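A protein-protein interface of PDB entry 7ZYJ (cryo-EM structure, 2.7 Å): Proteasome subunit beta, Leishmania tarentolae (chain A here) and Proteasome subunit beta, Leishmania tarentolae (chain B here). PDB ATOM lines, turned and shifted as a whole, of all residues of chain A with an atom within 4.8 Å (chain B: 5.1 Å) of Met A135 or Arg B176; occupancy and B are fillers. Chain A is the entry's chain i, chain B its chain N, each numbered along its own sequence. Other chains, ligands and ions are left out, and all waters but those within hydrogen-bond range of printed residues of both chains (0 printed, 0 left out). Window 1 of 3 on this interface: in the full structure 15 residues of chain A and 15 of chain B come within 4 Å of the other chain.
NH2 of Arg B176 is in hydrogen-bond range of SD of Met A135, at 3.7 Å.
The guanidinium group (NH2) of Arg B176 is in salt-bridge range of the side-chain carboxylate (OE2) of Glu A139, 2.7 Å away.
Among the printed residues, pairs that only touch across the chains: Ala A136 with Ile B141 (3.3 Å), Glu A139 with Tyr B175 (3.3 Å), Ala A136 with Val B172 (3.6 Å), Ile A132 with Ile B141 (3.7 Å) and Phe A124 with Tyr B211 (3.7 Å).
Of the printed residues of chain B, Phe A124 touches Tyr B211 (3.7 Å).
Of the printed residues of chain B, Ile A132 touches Ile B141.
Of chain B, only Arg B176 comes within 4 Å of Met A135.
Gln A137 touches none of the printed residues of chain B.
Printed residues of chain B within 4 Å of Glu A139: Tyr B175 (3.3 Å) and Arg B176 (2.7 Å).
Of the printed residues of chain A, Ile B141 touches Ile A132 (3.7 Å) and Ala A136 (3.3 Å).
Printed residues of chain A within 4 Å of Tyr B175: Glu A139.
Of the printed residues of chain A, Arg B176 touches Met A135 and Glu A139.
The nearest residue of chain A that does not touch Arg B176 is Phe A124 (4.3 Å).
The nearest printed residue of chain B that does not touch Glu A139 is Val B172 (4.02 Å).
Among the printed residues, 7 pairs touch across the chains.
Among the printed residues, Asp or Glu carboxylates within 4 Å of a Lys or Arg side-chain nitrogen of the other chain: Glu A139 with Arg B176 (2.7 Å).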
ATOM      1  N   PHE A 124      18.655  -0.503  -1.382  1.00  0.00           N
ATOM      2  CA  PHE A 124      18.000   0.790  -1.257  1.00  0.00           C
ATOM      3  C   PHE A 124      18.090   1.504  -2.595  1.00  0.00           C
ATOM      4  O   PHE A 124      19.140   1.496  -3.242  1.00  0.00           O
ATOM      5  CB  PHE A 124      18.619   1.648  -0.145  1.00  0.00           C
ATOM      6  CG  PHE A 124      20.109   1.813  -0.256  1.00  0.00           C
ATOM      7  CD1 PHE A 124      20.968   0.829   0.206  1.00  0.00           C
ATOM      8  CD2 PHE A 124      20.651   2.960  -0.809  1.00  0.00           C
ATOM      9  CE1 PHE A 124      22.335   0.983   0.107  1.00  0.00           C
ATOM     10  CE2 PHE A 124      22.018   3.120  -0.910  1.00  0.00           C
ATOM     11  CZ  PHE A 124      22.861   2.129  -0.451  1.00  0.00           C
ATOM     12  N   VAL A 125      16.977   2.114  -3.006  1.00  0.00           N
ATOM     13  CA  VAL A 125      16.848   2.703  -4.333  1.00  0.00           C
ATOM     14  C   VAL A 125      16.081   4.015  -4.247  1.00  0.00           C
ATOM     15  O   VAL A 125      15.261   4.228  -3.352  1.00  0.00           O
ATOM     16  CB  VAL A 125      16.140   1.753  -5.323  1.00  0.00           C
ATOM     17  CG1 VAL A 125      16.940   0.478  -5.534  1.00  0.00           C
ATOM     18  CG2 VAL A 125      14.735   1.431  -4.841  1.00  0.00           C
ATOM     19  N   THR A 126      16.353   4.895  -5.209  1.00  0.00           N
ATOM     20  CA  THR A 126      15.622   6.144  -5.368  1.00  0.00           C
ATOM     21  C   THR A 126      15.304   6.355  -6.840  1.00  0.00           C
ATOM     22  O   THR A 126      16.078   5.956  -7.714  1.00  0.00           O
ATOM     23  CB  THR A 126      16.415   7.351  -4.845  1.00  0.00           C
ATOM     24  OG1 THR A 126      17.689   7.410  -5.496  1.00  0.00           O
ATOM     25  CG2 THR A 126      16.617   7.257  -3.348  1.00  0.00           C
ATOM     26  N   SER A 131      15.328  12.304  -6.698  1.00  0.00           N
ATOM     27  CA  SER A 131      15.972  11.066  -6.277  1.00  0.00           C
ATOM     28  C   SER A 131      17.375  11.295  -5.733  1.00  0.00           C
ATOM     29  O   SER A 131      17.732  10.716  -4.700  1.00  0.00           O
ATOM     30  CB  SER A 131      16.025  10.082  -7.444  1.00  0.00           C
ATOM     31  OG  SER A 131      16.865  10.563  -8.477  1.00  0.00           O
ATOM     32  N   ILE A 132      18.171  12.135  -6.397  1.00  0.00           N
ATOM     33  CA  ILE A 132      19.564  12.311  -5.998  1.00  0.00           C
ATOM     34  C   ILE A 132      19.655  12.813  -4.564  1.00  0.00           C
ATOM     35  O   ILE A 132      20.348  12.220  -3.729  1.00  0.00           O
ATOM     36  CB  ILE A 132      20.280  13.255  -6.979  1.00  0.00           C
ATOM     37  CG1 ILE A 132      20.432  12.582  -8.345  1.00  0.00           C
ATOM     38  CG2 ILE A 132      21.633  13.671  -6.432  1.00  0.00           C
ATOM     39  CD1 ILE A 132      21.178  13.414  -9.359  1.00  0.00           C
ATOM     40  N   ALA A 133      18.921  13.881  -4.243  1.00  0.00           N
ATOM     41  CA  ALA A 133      18.900  14.375  -2.872  1.00  0.00           C
ATOM     42  C   ALA A 133      18.379  13.319  -1.909  1.00  0.00           C
ATOM     43  O   ALA A 133      18.801  13.278  -0.749  1.00  0.00           O
ATOM     44  CB  ALA A 133      18.055  15.644  -2.780  1.00  0.00           C
ATOM     45  N   ALA A 134      17.465  12.462  -2.367  1.00  0.00           N
ATOM     46  CA  ALA A 134      17.037  11.338  -1.542  1.00  0.00           C
ATOM     47  C   ALA A 134      18.167  10.332  -1.372  1.00  0.00           C
ATOM     48  O   ALA A 134      18.433   9.865  -0.258  1.00  0.00           O
ATOM     49  CB  ALA A 134      15.806  10.676  -2.157  1.00  0.00           C
ATOM     50  N   MET A 135      18.864  10.009  -2.465  1.00  0.00           N
ATOM     51  CA  MET A 135      19.895   8.979  -2.405  1.00  0.00           C
ATOM     52  C   MET A 135      21.016   9.378  -1.457  1.00  0.00           C
ATOM     53  O   MET A 135      21.513   8.546  -0.689  1.00  0.00           O
ATOM     54  CB  MET A 135      20.445   8.701  -3.803  1.00  0.00           C
ATOM     55  CG  MET A 135      21.570   7.681  -3.827  1.00  0.00           C
ATOM     56  SD  MET A 135      21.066   6.077  -3.178  1.00  0.00           S
ATOM     57  CE  MET A 135      20.153   5.416  -4.568  1.00  0.00           C
ATOM     58  N   ALA A 136      21.412  10.653  -1.485  1.00  0.00           N
ATOM     59  CA  ALA A 136      22.447  11.128  -0.575  1.00  0.00           C
ATOM     60  C   ALA A 136      22.072  10.876   0.877  1.00  0.00           C
ATOM     61  O   ALA A 136      22.954  10.662   1.716  1.00  0.00           O
ATOM     62  CB  ALA A 136      22.708  12.616  -0.807  1.00  0.00           C
ATOM     63  N   GLN A 137      20.776  10.890   1.197  1.00  0.00           N
ATOM     64  CA  GLN A 137      20.368  10.547   2.553  1.00  0.00           C
ATOM     65  C   GLN A 137      20.529   9.055   2.810  1.00  0.00           C
ATOM     66  O   GLN A 137      21.055   8.653   3.855  1.00  0.00           O
ATOM     67  CB  GLN A 137      18.926  10.989   2.798  1.00  0.00           C
ATOM     68  CG  GLN A 137      18.348  10.506   4.115  1.00  0.00           C
ATOM     69  CD  GLN A 137      18.943  11.221   5.310  1.00  0.00           C
ATOM     70  OE1 GLN A 137      19.576  12.266   5.171  1.00  0.00           O
ATOM     71  NE2 GLN A 137      18.741  10.661   6.496  1.00  0.00           N
ATOM     72  N   LEU A 138      20.108   8.220   1.857  1.00  0.00           N
ATOM     73  CA  LEU A 138      20.201   6.775   2.044  1.00  0.00           C
ATOM     74  C   LEU A 138      21.651   6.336   2.182  1.00  0.00           C
ATOM     75  O   LEU A 138      21.982   5.506   3.034  1.00  0.00           O
ATOM     76  CB  LEU A 138      19.525   6.047   0.883  1.00  0.00           C
ATOM     77  CG  LEU A 138      18.026   6.276   0.701  1.00  0.00           C
ATOM     78  CD1 LEU A 138      17.503   5.407  -0.425  1.00  0.00           C
ATOM     79  CD2 LEU A 138      17.279   5.991   1.989  1.00  0.00           C
ATOM     80  N   GLU A 139      22.537   6.894   1.355  1.00  0.00           N
ATOM     81  CA  GLU A 139      23.951   6.562   1.461  1.00  0.00           C
ATOM     82  C   GLU A 139      24.556   7.034   2.774  1.00  0.00           C
ATOM     83  O   GLU A 139      25.653   6.591   3.132  1.00  0.00           O
ATOM     84  CB  GLU A 139      24.723   7.164   0.286  1.00  0.00           C
ATOM     85  CG  GLU A 139      24.415   6.526  -1.058  1.00  0.00           C
ATOM     86  CD  GLU A 139      25.273   5.308  -1.344  1.00  0.00           C
ATOM     87  OE1 GLU A 139      25.822   4.723  -0.388  1.00  0.00           O
ATOM     88  OE2 GLU A 139      25.399   4.936  -2.528  1.00  0.00           O
ATOM     89  N   ILE B 141      23.862  16.750  -4.047  1.00  0.00           N
ATOM     90  CA  ILE B 141      24.154  15.615  -3.181  1.00  0.00           C
ATOM     91  C   ILE B 141      24.427  16.089  -1.759  1.00  0.00           C
ATOM     92  O   ILE B 141      23.698  15.740  -0.824  1.00  0.00           O
ATOM     93  CB  ILE B 141      25.343  14.806  -3.726  1.00  0.00           C
ATOM     94  CG1 ILE B 141      24.985  14.166  -5.068  1.00  0.00           C
ATOM     95  CG2 ILE B 141      25.774  13.750  -2.730  1.00  0.00           C
ATOM     96  CD1 ILE B 141      26.143  13.465  -5.738  1.00  0.00           C
ATOM     97  N   VAL B 172      29.611  10.476   0.567  1.00  0.00           N
ATOM     98  CA  VAL B 172      28.478  10.293  -0.338  1.00  0.00           C
ATOM     99  C   VAL B 172      28.817  10.792  -1.739  1.00  0.00           C
ATOM    100  O   VAL B 172      28.419  10.178  -2.738  1.00  0.00           O
ATOM    101  CB  VAL B 172      27.224  10.984   0.226  1.00  0.00           C
ATOM    102  CG1 VAL B 172      26.059  10.815  -0.726  1.00  0.00           C
ATOM    103  CG2 VAL B 172      26.873  10.410   1.587  1.00  0.00           C
ATOM    104  N   LEU B 173      29.560  11.899  -1.841  1.00  0.00           N
ATOM    105  CA  LEU B 173      29.974  12.402  -3.146  1.00  0.00           C
ATOM    106  C   LEU B 173      30.872  11.402  -3.861  1.00  0.00           C
ATOM    107  O   LEU B 173      30.730  11.181  -5.068  1.00  0.00           O
ATOM    108  CB  LEU B 173      30.691  13.742  -2.988  1.00  0.00           C
ATOM    109  CG  LEU B 173      29.819  14.992  -2.868  1.00  0.00           C
ATOM    110  CD1 LEU B 173      30.637  16.152  -2.330  1.00  0.00           C
ATOM    111  CD2 LEU B 173      29.204  15.346  -4.210  1.00  0.00           C
ATOM    112  N   PHE B 174      31.806  10.789  -3.132  1.00  0.00           N
ATOM    113  CA  PHE B 174      32.637   9.752  -3.730  1.00  0.00           C
ATOM    114  C   PHE B 174      31.805   8.554  -4.162  1.00  0.00           C
ATOM    115  O   PHE B 174      32.110   7.925  -5.182  1.00  0.00           O
ATOM    116  CB  PHE B 174      33.728   9.317  -2.752  1.00  0.00           C
ATOM    117  CG  PHE B 174      34.587   8.202  -3.267  1.00  0.00           C
ATOM    118  CD1 PHE B 174      35.326   8.357  -4.426  1.00  0.00           C
ATOM    119  CD2 PHE B 174      34.649   6.992  -2.598  1.00  0.00           C
ATOM    120  CE1 PHE B 174      36.115   7.331  -4.905  1.00  0.00           C
ATOM    121  CE2 PHE B 174      35.436   5.963  -3.072  1.00  0.00           C
ATOM    122  CZ  PHE B 174      36.169   6.132  -4.226  1.00  0.00           C
ATOM    123  N   TYR B 175      30.762   8.220  -3.400  1.00  0.00           N
ATOM    124  CA  TYR B 175      29.867   7.141  -3.805  1.00  0.00           C
ATOM    125  C   TYR B 175      29.153   7.465  -5.112  1.00  0.00           C
ATOM    126  O   TYR B 175      29.061   6.619  -6.008  1.00  0.00           O
ATOM    127  CB  TYR B 175      28.838   6.861  -2.707  1.00  0.00           C
ATOM    128  CG  TYR B 175      29.359   6.088  -1.520  1.00  0.00           C
ATOM    129  CD1 TYR B 175      30.421   5.205  -1.648  1.00  0.00           C
ATOM    130  CD2 TYR B 175      28.774   6.230  -0.271  1.00  0.00           C
ATOM    131  CE1 TYR B 175      30.892   4.495  -0.562  1.00  0.00           C
ATOM    132  CE2 TYR B 175      29.236   5.526   0.819  1.00  0.00           C
ATOM    133  CZ  TYR B 175      30.294   4.661   0.669  1.00  0.00           C
ATOM    134  OH  TYR B 175      30.753   3.960   1.758  1.00  0.00           O
ATOM    135  N   ARG B 176      28.642   8.690  -5.244  1.00  0.00           N
ATOM    136  CA  ARG B 176      27.631   8.985  -6.253  1.00  0.00           C
ATOM    137  C   ARG B 176      28.094   9.904  -7.377  1.00  0.00           C
ATOM    138  O   ARG B 176      27.320  10.141  -8.310  1.00  0.00           O
ATOM    139  CB  ARG B 176      26.392   9.586  -5.583  1.00  0.00           C
ATOM    140  CG  ARG B 176      25.585   8.573  -4.798  1.00  0.00           C
ATOM    141  CD  ARG B 176      25.123   7.442  -5.698  1.00  0.00           C
ATOM    142  NE  ARG B 176      24.829   6.230  -4.945  1.00  0.00           N
ATOM    143  CZ  ARG B 176      24.052   5.247  -5.379  1.00  0.00           C
ATOM    144  NH1 ARG B 176      23.465   5.302  -6.562  1.00  0.00           N
ATOM    145  NH2 ARG B 176      23.861   4.183  -4.606  1.00  0.00           N
ATOM    146  N   GLU B 177      29.315  10.425  -7.331  1.00  0.00           N
ATOM    147  CA  GLU B 177      29.827  11.288  -8.389  1.00  0.00           C
ATOM    148  C   GLU B 177      30.849  10.522  -9.217  1.00  0.00           C
ATOM    149  O   GLU B 177      31.777   9.922  -8.664  1.00  0.00           O
ATOM    150  CB  GLU B 177      30.448  12.563  -7.818  1.00  0.00           C
ATOM    151  CG  GLU B 177      30.720  13.636  -8.857  1.00  0.00           C
ATOM    152  CD  GLU B 177      31.653  14.717  -8.352  1.00  0.00           C
ATOM    153  OE1 GLU B 177      32.065  14.646  -7.176  1.00  0.00           O
ATOM    154  OE2 GLU B 177      31.976  15.637  -9.132  1.00  0.00           O
ATOM    155  N   CYS B 178      30.673  10.542 -10.538  1.00  0.00           N
ATOM    156  CA  CYS B 178      31.523   9.750 -11.420  1.00  0.00           C
ATOM    157  C   CYS B 178      32.949  10.284 -11.448  1.00  0.00           C
ATOM    158  O   CYS B 178      33.913   9.528 -11.289  1.00  0.00           O
ATOM    159  CB  CYS B 178      30.931   9.730 -12.830  1.00  0.00           C
ATOM    160  SG  CYS B 178      29.377   8.836 -12.960  1.00  0.00           S
ATOM    161  N   TYR B 211      24.564  -6.353  -2.086  1.00  0.00           N
ATOM    162  CA  TYR B 211      25.536  -6.066  -3.131  1.00  0.00           C
ATOM    163  C   TYR B 211      26.209  -7.319  -3.672  1.00  0.00           C
ATOM    164  O   TYR B 211      27.063  -7.211  -4.557  1.00  0.00           O
ATOM    165  CB  TYR B 211      26.610  -5.109  -2.604  1.00  0.00           C
ATOM    166  CG  TYR B 211      26.223  -3.648  -2.643  1.00  0.00           C
ATOM    167  CD1 TYR B 211      24.911  -3.261  -2.869  1.00  0.00           C
ATOM    168  CD2 TYR B 211      27.175  -2.655  -2.454  1.00  0.00           C
ATOM    169  CE1 TYR B 211      24.556  -1.927  -2.905  1.00  0.00           C
ATOM    170  CE2 TYR B 211      26.831  -1.319  -2.488  1.00  0.00           C
ATOM    171  CZ  TYR B 211      25.520  -0.960  -2.713  1.00  0.00           C
ATOM    172  OH  TYR B 211      25.171   0.369  -2.748  1.00  0.00           O
